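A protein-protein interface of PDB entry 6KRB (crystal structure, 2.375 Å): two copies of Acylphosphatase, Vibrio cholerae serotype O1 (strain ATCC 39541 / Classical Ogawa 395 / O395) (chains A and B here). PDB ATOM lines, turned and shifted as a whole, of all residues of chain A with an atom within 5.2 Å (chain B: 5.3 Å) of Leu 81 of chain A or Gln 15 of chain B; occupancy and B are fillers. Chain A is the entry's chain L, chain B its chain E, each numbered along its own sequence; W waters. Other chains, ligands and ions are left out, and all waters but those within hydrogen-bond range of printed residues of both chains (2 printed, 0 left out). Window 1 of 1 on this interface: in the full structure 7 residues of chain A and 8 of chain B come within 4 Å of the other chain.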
ATOM      1  N   GLN A   4       3.497   5.246 -16.259  1.00  0.00           N
ATOM      2  CA  GLN A   4       3.586   6.644 -16.650  1.00  0.00           C
ATOM      3  C   GLN A   4       2.172   7.204 -16.726  1.00  0.00           C
ATOM      4  O   GLN A   4       1.204   6.446 -16.748  1.00  0.00           O
ATOM      5  CB  GLN A   4       4.304   6.800 -17.991  1.00  0.00           C
ATOM      6  CG  GLN A   4       3.469   6.378 -19.186  1.00  0.00           C
ATOM      7  CD  GLN A   4       4.214   6.514 -20.500  1.00  0.00           C
ATOM      8  OE1 GLN A   4       5.429   6.322 -20.563  1.00  0.00           O
ATOM      9  NE2 GLN A   4       3.486   6.849 -21.559  1.00  0.00           N
ATOM     10  N   CYS A   5       2.049   8.526 -16.766  1.00  0.00           N
ATOM     11  CA  CYS A   5       0.735   9.157 -16.827  1.00  0.00           C
ATOM     12  C   CYS A   5       0.542   9.932 -18.128  1.00  0.00           C
ATOM     13  O   CYS A   5       1.416  10.687 -18.551  1.00  0.00           O
ATOM     14  CB  CYS A   5       0.531  10.089 -15.629  1.00  0.00           C
ATOM     15  SG  CYS A   5       0.523   9.256 -14.020  1.00  0.00           S
ATOM     16  N   TYR A  35      -8.270   9.960 -13.399  1.00  0.00           N
ATOM     17  CA  TYR A  35      -9.555  10.639 -13.266  1.00  0.00           C
ATOM     18  C   TYR A  35     -10.120  11.131 -14.595  1.00  0.00           C
ATOM     19  O   TYR A  35      -9.426  11.152 -15.612  1.00  0.00           O
ATOM     20  CB  TYR A  35      -9.433  11.825 -12.300  1.00  0.00           C
ATOM     21  CG  TYR A  35      -8.469  12.914 -12.739  1.00  0.00           C
ATOM     22  CD1 TYR A  35      -8.873  13.922 -13.608  1.00  0.00           C
ATOM     23  CD2 TYR A  35      -7.164  12.945 -12.266  1.00  0.00           C
ATOM     24  CE1 TYR A  35      -8.001  14.918 -14.004  1.00  0.00           C
ATOM     25  CE2 TYR A  35      -6.284  13.940 -12.655  1.00  0.00           C
ATOM     26  CZ  TYR A  35      -6.709  14.924 -13.523  1.00  0.00           C
ATOM     27  OH  TYR A  35      -5.841  15.917 -13.917  1.00  0.00           O
ATOM     28  N   VAL A  47      -7.147  11.830 -17.371  1.00  0.00           N
ATOM     29  CA  VAL A  47      -5.792  11.495 -16.953  1.00  0.00           C
ATOM     30  C   VAL A  47      -5.732  10.039 -16.513  1.00  0.00           C
ATOM     31  O   VAL A  47      -6.500   9.616 -15.649  1.00  0.00           O
ATOM     32  CB  VAL A  47      -5.310  12.406 -15.809  1.00  0.00           C
ATOM     33  CG1 VAL A  47      -4.042  11.852 -15.175  1.00  0.00           C
ATOM     34  CG2 VAL A  47      -5.084  13.816 -16.325  1.00  0.00           C
ATOM     35  N   SER A  79       2.253  15.318 -20.155  1.00  0.00           N
ATOM     36  CA  SER A  79       2.053  15.202 -18.717  1.00  0.00           C
ATOM     37  C   SER A  79       3.340  14.747 -18.038  1.00  0.00           C
ATOM     38  O   SER A  79       4.083  13.928 -18.580  1.00  0.00           O
ATOM     39  CB  SER A  79       0.912  14.230 -18.404  1.00  0.00           C
ATOM     40  OG  SER A  79       0.661  14.169 -17.010  1.00  0.00           O
ATOM     41  N   GLU A  80       3.604  15.289 -16.855  1.00  0.00           N
ATOM     42  CA  GLU A  80       4.771  14.894 -16.076  1.00  0.00           C
ATOM     43  C   GLU A  80       4.323  14.408 -14.704  1.00  0.00           C
ATOM     44  O   GLU A  80       5.091  14.410 -13.741  1.00  0.00           O
ATOM     45  CB  GLU A  80       5.760  16.055 -15.955  1.00  0.00           C
ATOM     46  CG  GLU A  80       6.177  16.636 -17.299  1.00  0.00           C
ATOM     47  CD  GLU A  80       7.255  17.692 -17.175  1.00  0.00           C
ATOM     48  OE1 GLU A  80       7.423  18.487 -18.125  1.00  0.00           O
ATOM     49  OE2 GLU A  80       7.938  17.723 -16.130  1.00  0.00           O
ATOM     50  N   LEU A  81       3.059  13.997 -14.636  1.00  0.00           N
ATOM     51  CA  LEU A  81       2.483  13.423 -13.427  1.00  0.00           C
ATOM     52  C   LEU A  81       3.162  12.107 -13.069  1.00  0.00           C
ATOM     53  O   LEU A  81       3.301  11.221 -13.913  1.00  0.00           O
ATOM     54  CB  LEU A  81       0.977  13.197 -13.602  1.00  0.00           C
ATOM     55  CG  LEU A  81       0.031  14.372 -13.341  1.00  0.00           C
ATOM     56  CD1 LEU A  81      -1.378  14.052 -13.817  1.00  0.00           C
ATOM     57  CD2 LEU A  81       0.026  14.716 -11.861  1.00  0.00           C
ATOM     58  N   GLU A  82       3.589  11.993 -11.818  1.00  0.00           N
ATOM     59  CA  GLU A  82       4.143  10.748 -11.305  1.00  0.00           C
ATOM     60  C   GLU A  82       3.442  10.385 -10.002  1.00  0.00           C
ATOM     61  O   GLU A  82       3.883   9.505  -9.263  1.00  0.00           O
ATOM     62  CB  GLU A  82       5.656  10.861 -11.099  1.00  0.00           C
ATOM     63  CG  GLU A  82       6.452  10.997 -12.391  1.00  0.00           C
ATOM     64  CD  GLU A  82       7.949  10.867 -12.178  1.00  0.00           C
ATOM     65  OE1 GLU A  82       8.602  11.890 -11.881  1.00  0.00           O
ATOM     66  OE2 GLU A  82       8.475   9.742 -12.311  1.00  0.00           O
ATOM     67  N   HIS A  83       2.341  11.080  -9.734  1.00  0.00           N
ATOM     68  CA  HIS A  83       1.531  10.833  -8.549  1.00  0.00           C
ATOM     69  C   HIS A  83       0.645   9.606  -8.741  1.00  0.00           C
ATOM     70  O   HIS A  83       0.125   9.370  -9.832  1.00  0.00           O
ATOM     71  CB  HIS A  83       0.678  12.062  -8.226  1.00  0.00           C
ATOM     72  CG  HIS A  83      -0.298  11.846  -7.112  1.00  0.00           C
ATOM     73  ND1 HIS A  83       0.092  11.684  -5.801  1.00  0.00           N
ATOM     74  CD2 HIS A  83      -1.650  11.769  -7.115  1.00  0.00           C
ATOM     75  CE1 HIS A  83      -0.977  11.515  -5.042  1.00  0.00           C
ATOM     76  NE2 HIS A  83      -2.047  11.564  -5.816  1.00  0.00           N
ATOM     77  N   TYR A  85      -2.666   7.979  -8.266  1.00  0.00           N
ATOM     78  CA  TYR A  85      -4.076   8.181  -7.961  1.00  0.00           C
ATOM     79  C   TYR A  85      -4.738   6.876  -7.538  1.00  0.00           C
ATOM     80  O   TYR A  85      -4.313   5.790  -7.934  1.00  0.00           O
ATOM     81  CB  TYR A  85      -4.813   8.775  -9.164  1.00  0.00           C
ATOM     82  CG  TYR A  85      -4.409  10.196  -9.485  1.00  0.00           C
ATOM     83  CD1 TYR A  85      -5.022  11.271  -8.853  1.00  0.00           C
ATOM     84  CD2 TYR A  85      -3.418  10.462 -10.418  1.00  0.00           C
ATOM     85  CE1 TYR A  85      -4.656  12.573  -9.143  1.00  0.00           C
ATOM     86  CE2 TYR A  85      -3.046  11.758 -10.714  1.00  0.00           C
ATOM     87  CZ  TYR A  85      -3.667  12.809 -10.074  1.00  0.00           C
ATOM     88  OH  TYR A  85      -3.297  14.101 -10.369  1.00  0.00           O
ATOM     89  N   GLY B  12      10.905  19.839  -8.685  1.00  0.00           N
ATOM     90  CA  GLY B  12      11.958  18.857  -8.502  1.00  0.00           C
ATOM     91  C   GLY B  12      11.404  17.451  -8.628  1.00  0.00           C
ATOM     92  O   GLY B  12      10.346  17.248  -9.224  1.00  0.00           O
ATOM     93  N   HIS B  13      12.115  16.474  -8.075  1.00  0.00           N
ATOM     94  CA  HIS B  13      11.597  15.113  -8.009  1.00  0.00           C
ATOM     95  C   HIS B  13      10.675  15.007  -6.800  1.00  0.00           C
ATOM     96  O   HIS B  13      11.062  14.479  -5.757  1.00  0.00           O
ATOM     97  CB  HIS B  13      12.735  14.096  -7.920  1.00  0.00           C
ATOM     98  CG  HIS B  13      12.309  12.687  -8.191  1.00  0.00           C
ATOM     99  ND1 HIS B  13      11.579  12.334  -9.306  1.00  0.00           N
ATOM    100  CD2 HIS B  13      12.510  11.544  -7.495  1.00  0.00           C
ATOM    101  CE1 HIS B  13      11.347  11.033  -9.283  1.00  0.00           C
ATOM    102  NE2 HIS B  13      11.901  10.530  -8.196  1.00  0.00           N
ATOM    103  N   VAL B  14       9.453  15.510  -6.949  1.00  0.00           N
ATOM    104  CA  VAL B  14       8.579  15.741  -5.803  1.00  0.00           C
ATOM    105  C   VAL B  14       7.252  14.987  -5.848  1.00  0.00           C
ATOM    106  O   VAL B  14       6.460  15.070  -4.908  1.00  0.00           O
ATOM    107  CB  VAL B  14       8.266  17.242  -5.659  1.00  0.00           C
ATOM    108  CG1 VAL B  14       9.518  18.010  -5.280  1.00  0.00           C
ATOM    109  CG2 VAL B  14       7.684  17.781  -6.953  1.00  0.00           C
ATOM    110  N   GLN B  15       7.000  14.261  -6.929  1.00  0.00           N
ATOM    111  CA  GLN B  15       5.757  13.505  -7.034  1.00  0.00           C
ATOM    112  C   GLN B  15       5.997  12.004  -6.940  1.00  0.00           C
ATOM    113  O   GLN B  15       6.959  11.480  -7.502  1.00  0.00           O
ATOM    114  CB  GLN B  15       5.031  13.837  -8.338  1.00  0.00           C
ATOM    115  CG  GLN B  15       4.471  15.246  -8.390  1.00  0.00           C
ATOM    116  CD  GLN B  15       3.456  15.420  -9.500  1.00  0.00           C
ATOM    117  OE1 GLN B  15       3.167  14.484 -10.243  1.00  0.00           O
ATOM    118  NE2 GLN B  15       2.906  16.622  -9.616  1.00  0.00           N
ATOM    119  N   GLY B  16       5.113  11.319  -6.222  1.00  0.00           N
ATOM    120  CA  GLY B  16       5.207   9.881  -6.071  1.00  0.00           C
ATOM    121  C   GLY B  16       6.338   9.466  -5.152  1.00  0.00           C
ATOM    122  O   GLY B  16       6.762   8.310  -5.164  1.00  0.00           O
ATOM    123  N   VAL B  17       6.829  10.406  -4.351  1.00  0.00           N
ATOM    124  CA  VAL B  17       7.942  10.131  -3.452  1.00  0.00           C
ATOM    125  C   VAL B  17       7.613  10.538  -2.015  1.00  0.00           C
ATOM    126  O   VAL B  17       8.507  10.857  -1.228  1.00  0.00           O
ATOM    127  CB  VAL B  17       9.226  10.849  -3.915  1.00  0.00           C
ATOM    128  CG1 VAL B  17       9.781  10.190  -5.171  1.00  0.00           C
ATOM    129  CG2 VAL B  17       8.948  12.318  -4.162  1.00  0.00           C
ATOM    130  N   ASN B  38      -0.843  17.791  -6.507  1.00  0.00           N
ATOM    131  CA  ASN B  38       0.051  17.379  -7.579  1.00  0.00           C
ATOM    132  C   ASN B  38      -0.342  18.043  -8.894  1.00  0.00           C
ATOM    133  O   ASN B  38      -1.472  17.897  -9.361  1.00  0.00           O
ATOM    134  CB  ASN B  38       0.044  15.856  -7.731  1.00  0.00           C
ATOM    135  CG  ASN B  38       0.524  15.144  -6.479  1.00  0.00           C
ATOM    136  OD1 ASN B  38      -0.271  14.803  -5.602  1.00  0.00           O
ATOM    137  ND2 ASN B  38       1.829  14.916  -6.391  1.00  0.00           N
ATOM    138  N   LEU B  39       0.589  18.787  -9.481  1.00  0.00           N
ATOM    139  CA  LEU B  39       0.321  19.480 -10.732  1.00  0.00           C
ATOM    140  C   LEU B  39       0.777  18.634 -11.917  1.00  0.00           C
ATOM    141  O   LEU B  39       1.662  17.786 -11.782  1.00  0.00           O
ATOM    142  CB  LEU B  39       1.003  20.851 -10.745  1.00  0.00           C
ATOM    143  CG  LEU B  39       0.563  21.827  -9.647  1.00  0.00           C
ATOM    144  CD1 LEU B  39       1.370  23.117  -9.708  1.00  0.00           C
ATOM    145  CD2 LEU B  39      -0.929  22.121  -9.738  1.00  0.00           C
ATOM    146  N   ASN B  40       0.162  18.867 -13.072  1.00  0.00           N
ATOM    147  CA  ASN B  40       0.414  18.066 -14.265  1.00  0.00           C
ATOM    148  C   ASN B  40       1.861  18.154 -14.742  1.00  0.00           C
ATOM    149  O   ASN B  40       2.376  17.221 -15.357  1.00  0.00           O
ATOM    150  CB  ASN B  40      -0.526  18.493 -15.395  1.00  0.00           C
ATOM    151  CG  ASN B  40      -0.477  17.551 -16.586  1.00  0.00           C
ATOM    152  OD1 ASN B  40      -0.501  16.331 -16.428  1.00  0.00           O
ATOM    153  ND2 ASN B  40      -0.397  18.117 -17.786  1.00  0.00           N
ATOM    154  N   ASN B  41       2.516  19.274 -14.447  1.00  0.00           N
ATOM    155  CA  ASN B  41       3.881  19.499 -14.907  1.00  0.00           C
ATOM    156  C   ASN B  41       4.927  18.875 -13.985  1.00  0.00           C
ATOM    157  O   ASN B  41       6.129  19.045 -14.188  1.00  0.00           O
ATOM    158  CB  ASN B  41       4.146  20.999 -15.065  1.00  0.00           C
ATOM    159  CG  ASN B  41       4.162  21.741 -13.740  1.00  0.00           C
ATOM    160  OD1 ASN B  41       3.716  21.228 -12.713  1.00  0.00           O
ATOM    161  ND2 ASN B  41       4.672  22.968 -13.763  1.00  0.00           N
ATOM    162  N   GLY B  42       4.460  18.155 -12.972  1.00  0.00           N
ATOM    163  CA  GLY B  42       5.348  17.460 -12.059  1.00  0.00           C
ATOM    164  C   GLY B  42       5.624  18.233 -10.785  1.00  0.00           C
ATOM    165  O   GLY B  42       6.336  17.754  -9.904  1.00  0.00           O
ATOM    166  N   ASP B  43       5.064  19.434 -10.686  1.00  0.00           N
ATOM    167  CA  ASP B  43       5.227  20.243  -9.485  1.00  0.00           C
ATOM    168  C   ASP B  43       4.190  19.876  -8.435  1.00  0.00           C
ATOM    169  O   ASP B  43       3.220  19.174  -8.721  1.00  0.00           O
ATOM    170  CB  ASP B  43       5.123  21.734  -9.814  1.00  0.00           C
ATOM    171  CG  ASP B  43       6.306  22.241 -10.613  1.00  0.00           C
ATOM    172  OD1 ASP B  43       7.294  21.492 -10.760  1.00  0.00           O
ATOM    173  OD2 ASP B  43       6.248  23.396 -11.084  1.00  0.00           O
ATOM    174  N   VAL B  44       4.408  20.353  -7.214  1.00  0.00           N
ATOM    175  CA  VAL B  44       3.434  20.197  -6.141  1.00  0.00           C
ATOM    176  C   VAL B  44       3.069  21.561  -5.579  1.00  0.00           C
ATOM    177  O   VAL B  44       3.930  22.291  -5.088  1.00  0.00           O
ATOM    178  CB  VAL B  44       3.958  19.303  -5.004  1.00  0.00           C
ATOM    179  CG1 VAL B  44       2.973  19.293  -3.841  1.00  0.00           C
ATOM    180  CG2 VAL B  44       4.208  17.893  -5.509  1.00  0.00           C
HETATM  181  O   HOH W   1       2.720  12.803  -5.412  1.00  0.00           O
HETATM  182  O   HOH W   2      -3.942  15.968  -8.962  1.00  0.00           O
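Water W2 lies within hydrogen-bond range of OH of Tyr 85 of chain A (2.4 Å) and O of Asn 38 of chain B (3.2 Å). Water W1 lies within hydrogen-bond range of the side-chain amide nitrogen of Asn 38 of chain B, a ring nitrogen (ND1) of His 83 of chain A and the backbone NH of Gly 16 of chain B.
Of the printed residues of chain B, Leu 81 of chain A touches Gln 15 (3.4 Å), Leu 39 (3.5 Å) and Asn 40 (3.4 Å). Of the printed residues of chain A, Gln 15 of chain B touches Glu 80 (3.99 Å), Leu 81 (3.4 Å), Glu 82 (3.0 Å) and His 83 (3.5 Å). Printed residues of chain A within 4 Å of Gly 16 of chain B: Glu 82 (3.5 Å). Of the printed residues of chain B, His 83 of chain A touches Gln 15 (3.5 Å) and Asn 38 (3.1 Å). Val 14 of chain B touches none of the printed residues of chain A. The nearest printed residue of chain A that does not touch Gln 15 of chain B is Tyr 85 of chain A (6.5 Å).
Of the 13 printed residues of chain B, 8 touch a printed residue of chain A. Printed residues of chain B that touch a printed residue of chain A: His 13, Gln 15, Gly 16, Asn 38, Leu 39, Asn 40, Asn 41 and Gly 42. Among the printed residues, 13 pairs touch across the chains.
No position is printed for both chains. Of the 13 pairs that touch across the chains among the printed residues, none has its exchanged pair printed and touching as well.
The backbone carbonyl oxygen (O) of Asn 40 of chain B lies within hydrogen-bond range of the backbone NH (N) of Glu 80 of chain A, at 2.7 Å. OE2 of Glu 80 of chain A sits close to O of Asn 41 of chain B (3.0 Å). The backbone NH (N) of Leu 81 of chain A lies within hydrogen-bond range of the backbone carbonyl oxygen (O) of Asn 40 of chain B. The side-chain hydroxyl (OG) of Ser 79 of chain A is in hydrogen-bond range of the side-chain amide oxygen (OD1) of Asn 40 of chain B (2.5 Å). The side-chain amide oxygen of Asn 38 of chain B lies within hydrogen-bond range of a ring nitrogen (ND1) of His 83 of chain A (3.1 Å). The side-chain amide oxygen (OE1) of Gln 15 of chain B is in hydrogen-bond range of the backbone NH (N) of Glu 82 of chain A (3.0 Å).
Among the printed residues, pairs that only touch across the chains: Glu 80 of chain A with Gln 15 of chain B (3.99 Å), Glu 80 of chain A with Gly 42 of chain B (3.5 Å), Leu 81 of chain A with Gln 15 of chain B (3.4 Å), Leu 81 of chain A with Leu 39 of chain B (3.5 Å), Glu 82 of chain A with His 13 of chain B (3.9 Å), Glu 82 of chain A with Gly 16 of chain B (3.5 Å) and His 83 of chain A with Gln 15 of chain B (3.5 Å).
The side-chain amide nitrogen (NE2) of Gln 15 of chain B is in hydrogen-bond range of the backbone carbonyl oxygen (O) of Asp 43 of chain B. The side-chain amide oxygen of Asn 41 of chain B sits at hydrogen-bond distance from the backbone NH of Asp 43 of chain B (3.0 Å). NE2 of Gln 15 of chain B lies within hydrogen-bond range of O of Leu 39 of chain B, at 2.8 Å. The side-chain hydroxyl of Ser 79 of chain A sits at hydrogen-bond distance from the backbone NH of Leu 81 of chain A (3.4 Å).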
